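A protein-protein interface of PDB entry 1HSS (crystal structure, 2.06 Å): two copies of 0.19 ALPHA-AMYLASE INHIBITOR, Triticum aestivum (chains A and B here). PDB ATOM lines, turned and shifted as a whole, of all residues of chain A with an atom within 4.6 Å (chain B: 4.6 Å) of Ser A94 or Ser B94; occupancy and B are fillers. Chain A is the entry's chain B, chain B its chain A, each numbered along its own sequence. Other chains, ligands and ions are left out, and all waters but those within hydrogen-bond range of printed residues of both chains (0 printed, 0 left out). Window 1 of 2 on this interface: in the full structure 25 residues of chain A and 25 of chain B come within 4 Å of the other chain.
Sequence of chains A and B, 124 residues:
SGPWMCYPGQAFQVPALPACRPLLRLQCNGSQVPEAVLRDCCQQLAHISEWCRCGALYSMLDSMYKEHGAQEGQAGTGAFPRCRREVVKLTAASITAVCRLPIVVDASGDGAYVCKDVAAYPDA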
ATOM      1  N   LEU A  90       9.631 -22.877 -10.752  1.00  0.00           N
ATOM      2  CA  LEU A  90       8.747 -23.978 -11.151  1.00  0.00           C
ATOM      3  C   LEU A  90       7.540 -23.524 -11.982  1.00  0.00           C
ATOM      4  O   LEU A  90       7.079 -24.237 -12.874  1.00  0.00           O
ATOM      5  CB  LEU A  90       8.246 -24.701  -9.909  1.00  0.00           C
ATOM      6  CG  LEU A  90       8.358 -26.217  -9.948  1.00  0.00           C
ATOM      7  CD1 LEU A  90       9.806 -26.651 -10.217  1.00  0.00           C
ATOM      8  CD2 LEU A  90       7.876 -26.752  -8.611  1.00  0.00           C
ATOM      9  N   THR A  91       6.964 -22.386 -11.605  1.00  0.00           N
ATOM     10  CA  THR A  91       5.846 -21.783 -12.347  1.00  0.00           C
ATOM     11  C   THR A  91       6.294 -21.262 -13.739  1.00  0.00           C
ATOM     12  O   THR A  91       5.688 -21.596 -14.760  1.00  0.00           O
ATOM     13  CB  THR A  91       5.196 -20.603 -11.545  1.00  0.00           C
ATOM     14  OG1 THR A  91       4.865 -21.017 -10.211  1.00  0.00           O
ATOM     15  CG2 THR A  91       3.940 -20.135 -12.224  1.00  0.00           C
ATOM     16  N   ALA A  92       7.435 -20.575 -13.791  1.00  0.00           N
ATOM     17  CA  ALA A  92       7.946 -20.091 -15.059  1.00  0.00           C
ATOM     18  C   ALA A  92       8.214 -21.271 -16.000  1.00  0.00           C
ATOM     19  O   ALA A  92       7.808 -21.234 -17.158  1.00  0.00           O
ATOM     20  CB  ALA A  92       9.215 -19.249 -14.846  1.00  0.00           C
ATOM     21  N   ALA A  93       8.711 -22.379 -15.447  1.00  0.00           N
ATOM     22  CA  ALA A  93       9.054 -23.581 -16.223  1.00  0.00           C
ATOM     23  C   ALA A  93       7.858 -24.315 -16.836  1.00  0.00           C
ATOM     24  O   ALA A  93       8.026 -25.120 -17.736  1.00  0.00           O
ATOM     25  CB  ALA A  93       9.867 -24.568 -15.358  1.00  0.00           C
ATOM     26  N   SER A  94       6.648 -24.011 -16.380  1.00  0.00           N
ATOM     27  CA  SER A  94       5.472 -24.712 -16.872  1.00  0.00           C
ATOM     28  C   SER A  94       4.381 -23.816 -17.481  1.00  0.00           C
ATOM     29  O   SER A  94       3.296 -24.292 -17.835  1.00  0.00           O
ATOM     30  CB  SER A  94       4.895 -25.531 -15.735  1.00  0.00           C
ATOM     31  OG  SER A  94       4.723 -24.724 -14.599  1.00  0.00           O
ATOM     32  N   ILE A  95       4.722 -22.555 -17.723  1.00  0.00           N
ATOM     33  CA  ILE A  95       3.796 -21.596 -18.330  1.00  0.00           C
ATOM     34  C   ILE A  95       3.399 -22.124 -19.714  1.00  0.00           C
ATOM     35  O   ILE A  95       2.244 -22.067 -20.123  1.00  0.00           O
ATOM     36  CB  ILE A  95       4.469 -20.196 -18.485  1.00  0.00           C
ATOM     37  CG1 ILE A  95       4.497 -19.463 -17.134  1.00  0.00           C
ATOM     38  CG2 ILE A  95       3.743 -19.386 -19.568  1.00  0.00           C
ATOM     39  CD1 ILE A  95       5.271 -18.154 -17.127  1.00  0.00           C
ATOM     40  N   THR A  96       4.345 -22.827 -20.311  1.00  0.00           N
ATOM     41  CA  THR A  96       4.247 -23.363 -21.647  1.00  0.00           C
ATOM     42  C   THR A  96       3.326 -24.603 -21.645  1.00  0.00           C
ATOM     43  O   THR A  96       2.423 -24.744 -22.483  1.00  0.00           O
ATOM     44  CB  THR A  96       5.697 -23.623 -22.099  1.00  0.00           C
ATOM     45  OG1 THR A  96       5.796 -23.614 -23.519  1.00  0.00           O
ATOM     46  CG2 THR A  96       6.222 -24.867 -21.527  1.00  0.00           C
ATOM     47  N   ALA A  97       3.317 -25.283 -20.506  1.00  0.00           N
ATOM     48  CA  ALA A  97       2.338 -26.342 -20.249  1.00  0.00           C
ATOM     49  C   ALA A  97       0.919 -25.819 -20.048  1.00  0.00           C
ATOM     50  O   ALA A  97      -0.026 -26.394 -20.583  1.00  0.00           O
ATOM     51  CB  ALA A  97       2.750 -27.170 -19.047  1.00  0.00           C
ATOM     52  N   VAL A  98       0.758 -24.739 -19.284  1.00  0.00           N
ATOM     53  CA  VAL A  98      -0.582 -24.185 -19.097  1.00  0.00           C
ATOM     54  C   VAL A  98      -1.137 -23.569 -20.385  1.00  0.00           C
ATOM     55  O   VAL A  98      -2.338 -23.674 -20.643  1.00  0.00           O
ATOM     56  CB  VAL A  98      -0.674 -23.175 -17.892  1.00  0.00           C
ATOM     57  CG1 VAL A  98       0.396 -23.458 -16.875  1.00  0.00           C
ATOM     58  CG2 VAL A  98      -0.590 -21.770 -18.359  1.00  0.00           C
ATOM     59  N   VAL A 114       7.276 -28.539 -20.908  1.00  0.00           N
ATOM     60  CA  VAL A 114       7.829 -28.088 -19.642  1.00  0.00           C
ATOM     61  C   VAL A 114       9.320 -27.754 -19.854  1.00  0.00           C
ATOM     62  O   VAL A 114       9.965 -28.365 -20.708  1.00  0.00           O
ATOM     63  CB  VAL A 114       7.596 -29.218 -18.617  1.00  0.00           C
ATOM     64  CG1 VAL A 114       8.896 -29.779 -18.114  1.00  0.00           C
ATOM     65  CG2 VAL A 114       6.666 -28.746 -17.525  1.00  0.00           C
ATOM     66  N   LEU B  90       8.637 -32.948 -13.517  1.00  0.00           N
ATOM     67  CA  LEU B  90       8.298 -31.555 -13.769  1.00  0.00           C
ATOM     68  C   LEU B  90       6.895 -31.410 -14.337  1.00  0.00           C
ATOM     69  O   LEU B  90       6.192 -30.460 -14.009  1.00  0.00           O
ATOM     70  CB  LEU B  90       9.288 -30.954 -14.740  1.00  0.00           C
ATOM     71  CG  LEU B  90       9.918 -29.636 -14.318  1.00  0.00           C
ATOM     72  CD1 LEU B  90      10.555 -29.772 -12.943  1.00  0.00           C
ATOM     73  CD2 LEU B  90      10.964 -29.252 -15.353  1.00  0.00           C
ATOM     74  N   THR B  91       6.495 -32.327 -15.209  1.00  0.00           N
ATOM     75  CA  THR B  91       5.137 -32.330 -15.793  1.00  0.00           C
ATOM     76  C   THR B  91       4.043 -32.680 -14.752  1.00  0.00           C
ATOM     77  O   THR B  91       3.082 -31.932 -14.541  1.00  0.00           O
ATOM     78  CB  THR B  91       5.056 -33.332 -16.988  1.00  0.00           C
ATOM     79  OG1 THR B  91       6.065 -33.003 -17.945  1.00  0.00           O
ATOM     80  CG2 THR B  91       3.695 -33.301 -17.662  1.00  0.00           C
ATOM     81  N   ALA B  92       4.302 -33.718 -13.973  1.00  0.00           N
ATOM     82  CA  ALA B  92       3.407 -34.075 -12.897  1.00  0.00           C
ATOM     83  C   ALA B  92       3.219 -32.920 -11.876  1.00  0.00           C
ATOM     84  O   ALA B  92       2.096 -32.638 -11.452  1.00  0.00           O
ATOM     85  CB  ALA B  92       3.922 -35.350 -12.212  1.00  0.00           C
ATOM     86  N   ALA B  93       4.295 -32.182 -11.584  1.00  0.00           N
ATOM     87  CA  ALA B  93       4.278 -31.063 -10.630  1.00  0.00           C
ATOM     88  C   ALA B  93       3.401 -29.882 -11.072  1.00  0.00           C
ATOM     89  O   ALA B  93       3.059 -29.022 -10.260  1.00  0.00           O
ATOM     90  CB  ALA B  93       5.717 -30.569 -10.379  1.00  0.00           C
ATOM     91  N   SER B  94       3.056 -29.805 -12.355  1.00  0.00           N
ATOM     92  CA  SER B  94       2.345 -28.627 -12.855  1.00  0.00           C
ATOM     93  C   SER B  94       1.021 -28.965 -13.541  1.00  0.00           C
ATOM     94  O   SER B  94       0.387 -28.101 -14.150  1.00  0.00           O
ATOM     95  CB  SER B  94       3.248 -27.873 -13.824  1.00  0.00           C
ATOM     96  OG  SER B  94       3.681 -28.748 -14.845  1.00  0.00           O
ATOM     97  N   ILE B  95       0.538 -30.183 -13.332  1.00  0.00           N
ATOM     98  CA  ILE B  95      -0.758 -30.617 -13.893  1.00  0.00           C
ATOM     99  C   ILE B  95      -1.923 -29.808 -13.307  1.00  0.00           C
ATOM    100  O   ILE B  95      -2.846 -29.385 -14.001  1.00  0.00           O
ATOM    101  CB  ILE B  95      -0.994 -32.124 -13.634  1.00  0.00           C
ATOM    102  CG1 ILE B  95      -0.083 -32.952 -14.543  1.00  0.00           C
ATOM    103  CG2 ILE B  95      -2.467 -32.477 -13.853  1.00  0.00           C
ATOM    104  CD1 ILE B  95      -0.221 -34.453 -14.340  1.00  0.00           C
ATOM    105  N   THR B  96      -1.683 -29.387 -12.080  1.00  0.00           N
ATOM    106  CA  THR B  96      -2.557 -28.552 -11.271  1.00  0.00           C
ATOM    107  C   THR B  96      -2.569 -27.063 -11.798  1.00  0.00           C
ATOM    108  O   THR B  96      -3.642 -26.474 -12.039  1.00  0.00           O
ATOM    109  CB  THR B  96      -2.058 -28.766  -9.781  1.00  0.00           C
ATOM    110  OG1 THR B  96      -3.131 -28.627  -8.858  1.00  0.00           O
ATOM    111  CG2 THR B  96      -0.915 -27.894  -9.438  1.00  0.00           C
ATOM    112  N   ALA B  97      -1.423 -26.613 -12.306  1.00  0.00           N
ATOM    113  CA  ALA B  97      -1.359 -25.357 -13.053  1.00  0.00           C
ATOM    114  C   ALA B  97      -2.085 -25.414 -14.415  1.00  0.00           C
ATOM    115  O   ALA B  97      -2.815 -24.491 -14.779  1.00  0.00           O
ATOM    116  CB  ALA B  97       0.101 -24.947 -13.256  1.00  0.00           C
ATOM    117  N   VAL B  98      -1.892 -26.486 -15.182  1.00  0.00           N
ATOM    118  CA  VAL B  98      -2.583 -26.561 -16.456  1.00  0.00           C
ATOM    119  C   VAL B  98      -4.096 -26.676 -16.274  1.00  0.00           C
ATOM    120  O   VAL B  98      -4.849 -26.044 -17.009  1.00  0.00           O
ATOM    121  CB  VAL B  98      -2.024 -27.687 -17.376  1.00  0.00           C
ATOM    122  CG1 VAL B  98      -0.539 -27.921 -17.077  1.00  0.00           C
ATOM    123  CG2 VAL B  98      -2.844 -28.952 -17.262  1.00  0.00           C
ATOM    124  N   VAL B 114       1.439 -25.074  -8.376  1.00  0.00           N
ATOM    125  CA  VAL B 114       2.556 -25.902  -8.769  1.00  0.00           C
ATOM    126  C   VAL B 114       3.001 -26.665  -7.501  1.00  0.00           C
ATOM    127  O   VAL B 114       2.838 -26.158  -6.381  1.00  0.00           O
ATOM    128  CB  VAL B 114       3.645 -24.955  -9.370  1.00  0.00           C
ATOM    129  CG1 VAL B 114       4.926 -25.042  -8.638  1.00  0.00           C
ATOM    130  CG2 VAL B 114       3.781 -25.187 -10.849  1.00  0.00           C
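The backbone carbonyl oxygen (O) of Leu B90 lies within hydrogen-bond range of the side-chain hydroxyl (OG) of Ser B94, at 3.2 Å.
The backbone carbonyl oxygen (O) of Thr B91 is in hydrogen-bond range of the side-chain hydroxyl (OG) of Ser B94.
The side-chain hydroxyl (OG) of Ser A94 is in hydrogen-bond range of the backbone carbonyl oxygen (O) of Leu A90, at 3.0 Å.
The side-chain hydroxyl (OG) of Ser A94 is in hydrogen-bond range of the backbone carbonyl oxygen (O) of Thr A91 (3.3 Å).
Leu A90 touches Val B114 (CD2 to CG1, 3.4 Å).
Ser B94 touches Ser A94 (CB to CB, 3.4 Å).
Ser A94 touches Val B114.
O of Ala A97 touches CG1 of Val B98 (3.9 Å).
Val A98 touches Ala B97 (CG1 to CB, 3.9 Å).
CG1 of Val A114 touches CD2 of Leu B90, at 3.5 Å.
Printed residues of chain B within 4 Å of Leu A90: Val B114 (3.4 Å).
Thr A91 touches none of the printed residues of chain B.
Ser A94 touches just these residues of chain B: Ser B94 (3.4 Å) and Val B114 (3.9 Å).
Thr A96 touches none of the printed residues of chain B.
Printed residues of chain B within 4 Å of Val A114: Leu B90.
Printed residues of chain A within 4 Å of Ser B94: Ser A94.
Of the printed residues of chain A, Ala B97 touches Val A98.
Of the printed residues of chain A, Val B114 touches Leu A90 (3.4 Å) and Ser A94 (3.9 Å).
The nearest printed residue of chain B that does not touch Ser A94 is Ala B97 (4.8 Å).
Of the 10 printed residues of chain B, 5 touch a printed residue of chain A.
Printed residues of chain B that touch a printed residue of chain A: Leu B90, Ser B94, Ala B97, Val B98 and Val B114.
Among the printed residues, 6 pairs touch across the chains.
Leu A90 touches Val B114, and with the chains exchanged Val A114 touches Leu B90.
Ser B94 touches its own counterpart, Ser A94.
Ser A94 touches Val B114, but with the chains exchanged Val A114 does not touch Ser B94 (4.01 Å).
Ala A97 touches Val B98, and with the chains exchanged Val A98 touches Ala B97.
10 positions are printed for both chains.
Of the 6 pairs that touch across the chains among the printed residues, 5 have their exchanged pair printed and touching as well.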
